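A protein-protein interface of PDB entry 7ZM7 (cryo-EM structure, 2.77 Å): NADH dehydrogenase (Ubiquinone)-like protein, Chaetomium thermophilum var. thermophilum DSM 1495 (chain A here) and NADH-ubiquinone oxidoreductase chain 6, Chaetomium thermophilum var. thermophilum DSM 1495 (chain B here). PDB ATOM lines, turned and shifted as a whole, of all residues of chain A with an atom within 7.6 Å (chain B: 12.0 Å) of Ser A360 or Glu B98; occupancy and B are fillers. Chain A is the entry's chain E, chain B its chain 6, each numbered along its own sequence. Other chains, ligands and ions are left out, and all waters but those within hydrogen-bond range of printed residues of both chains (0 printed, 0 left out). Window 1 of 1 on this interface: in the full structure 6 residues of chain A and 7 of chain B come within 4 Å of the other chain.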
ATOM      1  N   TYR A 355      32.940  13.248 -11.076  1.00  0.00           N
ATOM      2  CA  TYR A 355      33.405  12.518  -9.902  1.00  0.00           C
ATOM      3  C   TYR A 355      32.797  13.076  -8.618  1.00  0.00           C
ATOM      4  O   TYR A 355      32.293  12.319  -7.781  1.00  0.00           O
ATOM      5  CB  TYR A 355      34.931  12.554  -9.838  1.00  0.00           C
ATOM      6  N   LEU A 357      30.172  14.456  -7.844  1.00  0.00           N
ATOM      7  CA  LEU A 357      28.693  14.486  -7.736  1.00  0.00           C
ATOM      8  C   LEU A 357      28.246  13.641  -6.543  1.00  0.00           C
ATOM      9  O   LEU A 357      29.001  12.739  -6.147  1.00  0.00           O
ATOM     10  CB  LEU A 357      28.111  13.959  -9.047  1.00  0.00           C
ATOM     11  CG  LEU A 357      28.353  14.842 -10.269  1.00  0.00           C
ATOM     12  CD1 LEU A 357      27.722  14.228 -11.506  1.00  0.00           C
ATOM     13  CD2 LEU A 357      27.813  16.244 -10.039  1.00  0.00           C
ATOM     14  N   PRO A 358      27.049  13.881  -5.966  1.00  0.00           N
ATOM     15  CA  PRO A 358      26.602  13.163  -4.775  1.00  0.00           C
ATOM     16  C   PRO A 358      26.228  11.702  -5.062  1.00  0.00           C
ATOM     17  O   PRO A 358      25.995  11.368  -6.210  1.00  0.00           O
ATOM     18  CB  PRO A 358      25.364  13.960  -4.349  1.00  0.00           C
ATOM     19  CG  PRO A 358      24.822  14.510  -5.641  1.00  0.00           C
ATOM     20  CD  PRO A 358      26.066  14.871  -6.422  1.00  0.00           C
ATOM     21  N   PRO A 359      26.181  10.815  -4.043  1.00  0.00           N
ATOM     22  CA  PRO A 359      25.777   9.426  -4.251  1.00  0.00           C
ATOM     23  C   PRO A 359      24.345   9.403  -4.795  1.00  0.00           C
ATOM     24  O   PRO A 359      23.542  10.195  -4.335  1.00  0.00           O
ATOM     25  CB  PRO A 359      25.879   8.798  -2.858  1.00  0.00           C
ATOM     26  CG  PRO A 359      26.849   9.691  -2.122  1.00  0.00           C
ATOM     27  CD  PRO A 359      26.559  11.079  -2.653  1.00  0.00           C
ATOM     28  N   SER A 360      24.056   8.507  -5.738  1.00  0.00           N
ATOM     29  CA  SER A 360      22.730   8.501  -6.415  1.00  0.00           C
ATOM     30  C   SER A 360      21.592   7.983  -5.534  1.00  0.00           C
ATOM     31  O   SER A 360      21.874   7.254  -4.564  1.00  0.00           O
ATOM     32  CB  SER A 360      22.799   7.737  -7.699  1.00  0.00           C
ATOM     33  OG  SER A 360      23.212   6.405  -7.450  1.00  0.00           O
ATOM     34  N   THR A 361      20.351   8.347  -5.880  1.00  0.00           N
ATOM     35  CA  THR A 361      19.157   7.899  -5.118  1.00  0.00           C
ATOM     36  C   THR A 361      18.571   6.641  -5.757  1.00  0.00           C
ATOM     37  O   THR A 361      18.908   6.372  -6.916  1.00  0.00           O
ATOM     38  CB  THR A 361      18.071   8.979  -5.115  1.00  0.00           C
ATOM     39  OG1 THR A 361      17.408   8.944  -6.379  1.00  0.00           O
ATOM     40  CG2 THR A 361      18.613  10.365  -4.844  1.00  0.00           C
ATOM     41  N   GLU A 362      17.689   5.937  -5.049  1.00  0.00           N
ATOM     42  CA  GLU A 362      17.099   4.689  -5.518  1.00  0.00           C
ATOM     43  C   GLU A 362      16.193   4.916  -6.724  1.00  0.00           C
ATOM     44  O   GLU A 362      16.065   4.042  -7.587  1.00  0.00           O
ATOM     45  CB  GLU A 362      16.331   4.013  -4.382  1.00  0.00           C
ATOM     46  CG  GLU A 362      15.098   4.764  -3.904  1.00  0.00           C
ATOM     47  CD  GLU A 362      13.828   4.268  -4.569  1.00  0.00           C
ATOM     48  OE1 GLU A 362      13.858   3.160  -5.142  1.00  0.00           O
ATOM     49  OE2 GLU A 362      12.801   4.976  -4.517  1.00  0.00           O
ATOM     50  N   LYS A 363      15.549   6.080  -6.797  1.00  0.00           N
ATOM     51  CA  LYS A 363      14.648   6.342  -7.912  1.00  0.00           C
ATOM     52  C   LYS A 363      15.420   6.410  -9.218  1.00  0.00           C
ATOM     53  O   LYS A 363      15.003   5.843 -10.233  1.00  0.00           O
ATOM     54  CB  LYS A 363      13.865   7.635  -7.664  1.00  0.00           C
ATOM     55  CG  LYS A 363      12.863   7.999  -8.760  1.00  0.00           C
ATOM     56  CD  LYS A 363      13.444   8.939  -9.806  1.00  0.00           C
ATOM     57  CE  LYS A 363      13.667  10.331  -9.246  1.00  0.00           C
ATOM     58  NZ  LYS A 363      14.222  11.251 -10.277  1.00  0.00           N
ATOM     59  N   GLU A 364      16.574   7.086  -9.194  1.00  0.00           N
ATOM     60  CA  GLU A 364      17.366   7.254 -10.441  1.00  0.00           C
ATOM     61  C   GLU A 364      18.177   5.987 -10.721  1.00  0.00           C
ATOM     62  O   GLU A 364      18.500   5.756 -11.895  1.00  0.00           O
ATOM     63  CB  GLU A 364      18.195   8.540 -10.418  1.00  0.00           C
ATOM     64  CG  GLU A 364      19.128   8.662  -9.231  1.00  0.00           C
ATOM     65  CD  GLU A 364      19.786  10.025  -9.107  1.00  0.00           C
ATOM     66  OE1 GLU A 364      19.799  10.765 -10.110  1.00  0.00           O
ATOM     67  OE2 GLU A 364      20.273  10.349  -8.007  1.00  0.00           O
ATOM     68  N   MET A 365      18.488   5.201  -9.692  1.00  0.00           N
ATOM     69  CA  MET A 365      19.186   3.905  -9.912  1.00  0.00           C
ATOM     70  C   MET A 365      18.261   3.024 -10.750  1.00  0.00           C
ATOM     71  O   MET A 365      18.771   2.284 -11.602  1.00  0.00           O
ATOM     72  CB  MET A 365      19.493   3.203  -8.588  1.00  0.00           C
ATOM     73  CG  MET A 365      20.702   3.766  -7.871  1.00  0.00           C
ATOM     74  SD  MET A 365      22.239   3.484  -8.786  1.00  0.00           S
ATOM     75  CE  MET A 365      22.316   1.695  -8.754  1.00  0.00           C
ATOM     76  N   GLU A 368      18.296   3.795 -14.529  1.00  0.00           N
ATOM     77  CA  GLU A 368      19.460   3.231 -15.251  1.00  0.00           C
ATOM     78  C   GLU A 368      19.114   1.839 -15.787  1.00  0.00           C
ATOM     79  O   GLU A 368      19.789   1.397 -16.710  1.00  0.00           O
ATOM     80  CB  GLU A 368      20.683   3.225 -14.335  1.00  0.00           C
ATOM     81  CG  GLU A 368      20.965   4.567 -13.689  1.00  0.00           C
ATOM     82  CD  GLU A 368      21.390   5.689 -14.621  1.00  0.00           C
ATOM     83  OE1 GLU A 368      21.152   6.861 -14.272  1.00  0.00           O
ATOM     84  OE2 GLU A 368      21.973   5.396 -15.681  1.00  0.00           O
ATOM     85  N   SER B  40      43.186   4.988  -1.343  1.00  0.00           N
ATOM     86  CA  SER B  40      42.817   6.012  -2.304  1.00  0.00           C
ATOM     87  C   SER B  40      41.324   5.986  -2.595  1.00  0.00           C
ATOM     88  O   SER B  40      40.721   4.919  -2.750  1.00  0.00           O
ATOM     89  CB  SER B  40      43.599   5.806  -3.595  1.00  0.00           C
ATOM     90  OG  SER B  40      43.451   6.906  -4.462  1.00  0.00           O
ATOM     91  N   LYS B  41      40.728   7.175  -2.681  1.00  0.00           N
ATOM     92  CA  LYS B  41      39.300   7.287  -2.955  1.00  0.00           C
ATOM     93  C   LYS B  41      38.972   6.916  -4.395  1.00  0.00           C
ATOM     94  O   LYS B  41      38.005   6.193  -4.651  1.00  0.00           O
ATOM     95  CB  LYS B  41      38.822   8.708  -2.657  1.00  0.00           C
ATOM     96  CG  LYS B  41      38.439   8.965  -1.210  1.00  0.00           C
ATOM     97  CD  LYS B  41      39.631   9.387  -0.372  1.00  0.00           C
ATOM     98  CE  LYS B  41      39.186   9.831   1.014  1.00  0.00           C
ATOM     99  NZ  LYS B  41      40.336  10.156   1.902  1.00  0.00           N
ATOM    100  N   ASN B  42      39.749   7.399  -5.332  1.00  0.00           N
ATOM    101  CA  ASN B  42      39.446   7.227  -6.745  1.00  0.00           C
ATOM    102  C   ASN B  42      40.051   5.938  -7.272  1.00  0.00           C
ATOM    103  O   ASN B  42      41.255   5.715  -7.108  1.00  0.00           O
ATOM    104  CB  ASN B  42      39.977   8.392  -7.552  1.00  0.00           C
ATOM    105  CG  ASN B  42      39.709   8.242  -9.018  1.00  0.00           C
ATOM    106  OD1 ASN B  42      38.743   7.616  -9.427  1.00  0.00           O
ATOM    107  ND2 ASN B  42      40.576   8.812  -9.823  1.00  0.00           N
ATOM    108  N   PRO B  43      39.266   5.077  -7.914  1.00  0.00           N
ATOM    109  CA  PRO B  43      39.844   3.857  -8.482  1.00  0.00           C
ATOM    110  C   PRO B  43      40.884   4.102  -9.561  1.00  0.00           C
ATOM    111  O   PRO B  43      41.748   3.242  -9.760  1.00  0.00           O
ATOM    112  CB  PRO B  43      38.629   3.109  -9.028  1.00  0.00           C
ATOM    113  CG  PRO B  43      37.464   3.763  -8.494  1.00  0.00           C
ATOM    114  CD  PRO B  43      37.802   5.051  -7.883  1.00  0.00           C
ATOM    115  N   ILE B  92      33.717   3.211 -17.677  1.00  0.00           N
ATOM    116  CA  ILE B  92      32.655   3.054 -16.701  1.00  0.00           C
ATOM    117  C   ILE B  92      32.420   4.378 -15.999  1.00  0.00           C
ATOM    118  O   ILE B  92      33.363   5.097 -15.646  1.00  0.00           O
ATOM    119  CB  ILE B  92      33.016   1.943 -15.705  1.00  0.00           C
ATOM    120  CG1 ILE B  92      32.856   0.578 -16.364  1.00  0.00           C
ATOM    121  CG2 ILE B  92      32.199   2.058 -14.455  1.00  0.00           C
ATOM    122  CD1 ILE B  92      32.999  -0.569 -15.401  1.00  0.00           C
ATOM    123  N   ASN B  93      31.157   4.733 -15.833  1.00  0.00           N
ATOM    124  CA  ASN B  93      30.827   5.901 -15.039  1.00  0.00           C
ATOM    125  C   ASN B  93      31.062   5.580 -13.574  1.00  0.00           C
ATOM    126  O   ASN B  93      30.538   4.593 -13.058  1.00  0.00           O
ATOM    127  CB  ASN B  93      29.386   6.321 -15.297  1.00  0.00           C
ATOM    128  CG  ASN B  93      29.203   6.931 -16.663  1.00  0.00           C
ATOM    129  OD1 ASN B  93      28.579   6.342 -17.542  1.00  0.00           O
ATOM    130  ND2 ASN B  93      29.754   8.123 -16.855  1.00  0.00           N
ATOM    131  N   ILE B  94      31.873   6.387 -12.911  1.00  0.00           N
ATOM    132  CA  ILE B  94      32.208   6.182 -11.512  1.00  0.00           C
ATOM    133  C   ILE B  94      31.916   7.466 -10.762  1.00  0.00           C
ATOM    134  O   ILE B  94      32.564   8.493 -10.996  1.00  0.00           O
ATOM    135  CB  ILE B  94      33.675   5.769 -11.328  1.00  0.00           C
ATOM    136  CG1 ILE B  94      33.954   4.438 -12.020  1.00  0.00           C
ATOM    137  CG2 ILE B  94      34.009   5.681  -9.857  1.00  0.00           C
ATOM    138  CD1 ILE B  94      35.276   4.386 -12.726  1.00  0.00           C
ATOM    139  N   ARG B  95      30.950   7.409  -9.860  1.00  0.00           N
ATOM    140  CA  ARG B  95      30.712   8.482  -8.908  1.00  0.00           C
ATOM    141  C   ARG B  95      31.560   8.168  -7.686  1.00  0.00           C
ATOM    142  O   ARG B  95      31.318   7.173  -6.997  1.00  0.00           O
ATOM    143  CB  ARG B  95      29.231   8.555  -8.567  1.00  0.00           C
ATOM    144  CG  ARG B  95      28.342   8.977  -9.718  1.00  0.00           C
ATOM    145  CD  ARG B  95      26.895   9.037  -9.256  1.00  0.00           C
ATOM    146  NE  ARG B  95      25.967   9.347 -10.334  1.00  0.00           N
ATOM    147  CZ  ARG B  95      25.618  10.577 -10.686  1.00  0.00           C
ATOM    148  NH1 ARG B  95      24.764  10.767 -11.681  1.00  0.00           N
ATOM    149  NH2 ARG B  95      26.106  11.616 -10.027  1.00  0.00           N
ATOM    150  N   THR B  96      32.566   9.000  -7.426  1.00  0.00           N
ATOM    151  CA  THR B  96      33.634   8.610  -6.514  1.00  0.00           C
ATOM    152  C   THR B  96      33.196   8.609  -5.064  1.00  0.00           C
ATOM    153  O   THR B  96      33.971   8.193  -4.200  1.00  0.00           O
ATOM    154  CB  THR B  96      34.842   9.530  -6.690  1.00  0.00           C
ATOM    155  OG1 THR B  96      35.989   8.954  -6.050  1.00  0.00           O
ATOM    156  CG2 THR B  96      34.571  10.890  -6.073  1.00  0.00           C
ATOM    157  N   SER B  97      31.993   9.082  -4.781  1.00  0.00           N
ATOM    158  CA  SER B  97      31.448   9.072  -3.436  1.00  0.00           C
ATOM    159  C   SER B  97      30.597   7.845  -3.142  1.00  0.00           C
ATOM    160  O   SER B  97      30.413   7.501  -1.971  1.00  0.00           O
ATOM    161  CB  SER B  97      30.655  10.351  -3.235  1.00  0.00           C
ATOM    162  OG  SER B  97      29.670  10.442  -4.242  1.00  0.00           O
ATOM    163  N   GLU B  98      30.083   7.169  -4.158  1.00  0.00           N
ATOM    164  CA  GLU B  98      29.388   5.914  -3.916  1.00  0.00           C
ATOM    165  C   GLU B  98      30.340   4.753  -3.640  1.00  0.00           C
ATOM    166  O   GLU B  98      29.897   3.711  -3.153  1.00  0.00           O
ATOM    167  CB  GLU B  98      28.487   5.568  -5.098  1.00  0.00           C
ATOM    168  CG  GLU B  98      27.585   6.687  -5.541  1.00  0.00           C
ATOM    169  CD  GLU B  98      26.972   6.441  -6.912  1.00  0.00           C
ATOM    170  OE1 GLU B  98      27.686   5.978  -7.820  1.00  0.00           O
ATOM    171  OE2 GLU B  98      25.769   6.710  -7.087  1.00  0.00           O
ATOM    172  N   LEU B  99      31.626   4.900  -3.933  1.00  0.00           N
ATOM    173  CA  LEU B  99      32.597   3.871  -3.610  1.00  0.00           C
ATOM    174  C   LEU B  99      33.271   4.115  -2.275  1.00  0.00           C
ATOM    175  O   LEU B  99      34.087   3.298  -1.845  1.00  0.00           O
ATOM    176  CB  LEU B  99      33.651   3.764  -4.709  1.00  0.00           C
ATOM    177  CG  LEU B  99      33.132   3.286  -6.055  1.00  0.00           C
ATOM    178  CD1 LEU B  99      34.283   2.928  -6.969  1.00  0.00           C
ATOM    179  CD2 LEU B  99      32.217   2.113  -5.892  1.00  0.00           C
ATOM    180  N   GLN B 100      32.926   5.197  -1.601  1.00  0.00           N
ATOM    181  CA  GLN B 100      33.587   5.586  -0.371  1.00  0.00           C
ATOM    182  C   GLN B 100      32.792   5.044   0.804  1.00  0.00           C
ATOM    183  O   GLN B 100      31.604   5.347   0.953  1.00  0.00           O
ATOM    184  CB  GLN B 100      33.726   7.106  -0.282  1.00  0.00           C
ATOM    185  CG  GLN B 100      34.467   7.562   0.950  1.00  0.00           C
ATOM    186  CD  GLN B 100      35.787   6.843   1.113  1.00  0.00           C
ATOM    187  OE1 GLN B 100      36.509   6.617   0.143  1.00  0.00           O
ATOM    188  NE2 GLN B 100      36.105   6.466   2.345  1.00  0.00           N
ATOM    189  N   SER B 101      33.450   4.252   1.635  1.00  0.00           N
ATOM    190  CA  SER B 101      32.847   3.686   2.826  1.00  0.00           C
ATOM    191  C   SER B 101      33.532   4.263   4.054  1.00  0.00           C
ATOM    192  O   SER B 101      34.640   4.798   3.984  1.00  0.00           O
ATOM    193  CB  SER B 101      32.949   2.162   2.816  1.00  0.00           C
ATOM    194  OG  SER B 101      34.290   1.744   2.915  1.00  0.00           O
ATOM    195  N   ASN B 102      32.857   4.141   5.191  1.00  0.00           N
ATOM    196  CA  ASN B 102      33.395   4.648   6.448  1.00  0.00           C
ATOM    197  C   ASN B 102      34.581   3.785   6.837  1.00  0.00           C
ATOM    198  O   ASN B 102      34.424   2.729   7.450  1.00  0.00           O
ATOM    199  CB  ASN B 102      32.322   4.634   7.528  1.00  0.00           C
ATOM    200  CG  ASN B 102      31.250   5.667   7.290  1.00  0.00           C
ATOM    201  OD1 ASN B 102      31.544   6.839   7.064  1.00  0.00           O
ATOM    202  ND2 ASN B 102      29.993   5.242   7.338  1.00  0.00           N
ATOM    203  N   THR B 103      35.780   4.244   6.486  1.00  0.00           N
ATOM    204  CA  THR B 103      36.982   3.460   6.727  1.00  0.00           C
ATOM    205  C   THR B 103      37.387   3.467   8.190  1.00  0.00           C
ATOM    206  O   THR B 103      38.091   2.556   8.637  1.00  0.00           O
ATOM    207  CB  THR B 103      38.131   3.999   5.884  1.00  0.00           C
ATOM    208  OG1 THR B 103      38.215   5.415   6.066  1.00  0.00           O
ATOM    209  CG2 THR B 103      37.900   3.694   4.415  1.00  0.00           C
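The backbone carbonyl oxygen (O) of Tyr A355 sits close to the backbone NH (N) of Thr B96.
O of Leu A357 sits at hydrogen-bond distance from OG of Ser B97.
OE2 of Glu B98 sits at hydrogen-bond distance from OG of Ser A360, at 2.6 Å.
OG of Ser A360 is in hydrogen-bond range of SD of Met A365.
NH2 of Arg B95 touches CB of Leu A357, 3.2 Å away.
O of Pro A358 touches NH2 of Arg B95 (3.8 Å).
Pro A358 touches Ser B97.
N of Pro A359 touches OG of Ser B97, 3.5 Å away.
Glu B98 touches Pro A359.
Of the printed residues of chain B, Leu A357 touches Arg B95 and Ser B97.
Of chain B, only Arg B95 and Ser B97 come within 4 Å of Pro A358.
Pro A359 touches just these residues of chain B: Ser B97 (3.5 Å) and Glu B98 (3.5 Å).
Printed residues of chain B within 4 Å of Ser A360: Glu B98 (2.6 Å).
No residue of chain B comes within 4 Å of Thr A361.
Of the printed residues of chain A, Arg B95 touches Leu A357 and Pro A358.
Glu B98 touches just these residues of chain A: Pro A359 and Ser A360.
The nearest residue of chain A that does not touch Glu B98 is Pro A358 (4.7 Å).
The nearest printed residue of chain A that does not touch Arg B95 is Tyr A355 (4.2 Å).
Of the 16 printed residues of chain B, 4 touch a printed residue of chain A.
Printed residues of chain A that touch a printed residue of chain B: Tyr A355, Leu A357, Pro A358, Pro A359 and Ser A360.
Hydrophobic or aromatic side chains of chain A within 4 Å of the printed part of chain B: Leu A357 and Pro A359.
Among the printed residues, 8 pairs touch across the chains.
Among the printed residues, no Asp or Glu carboxylate lies within 4 Å of a Lys or Arg side-chain nitrogen of the other chain.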
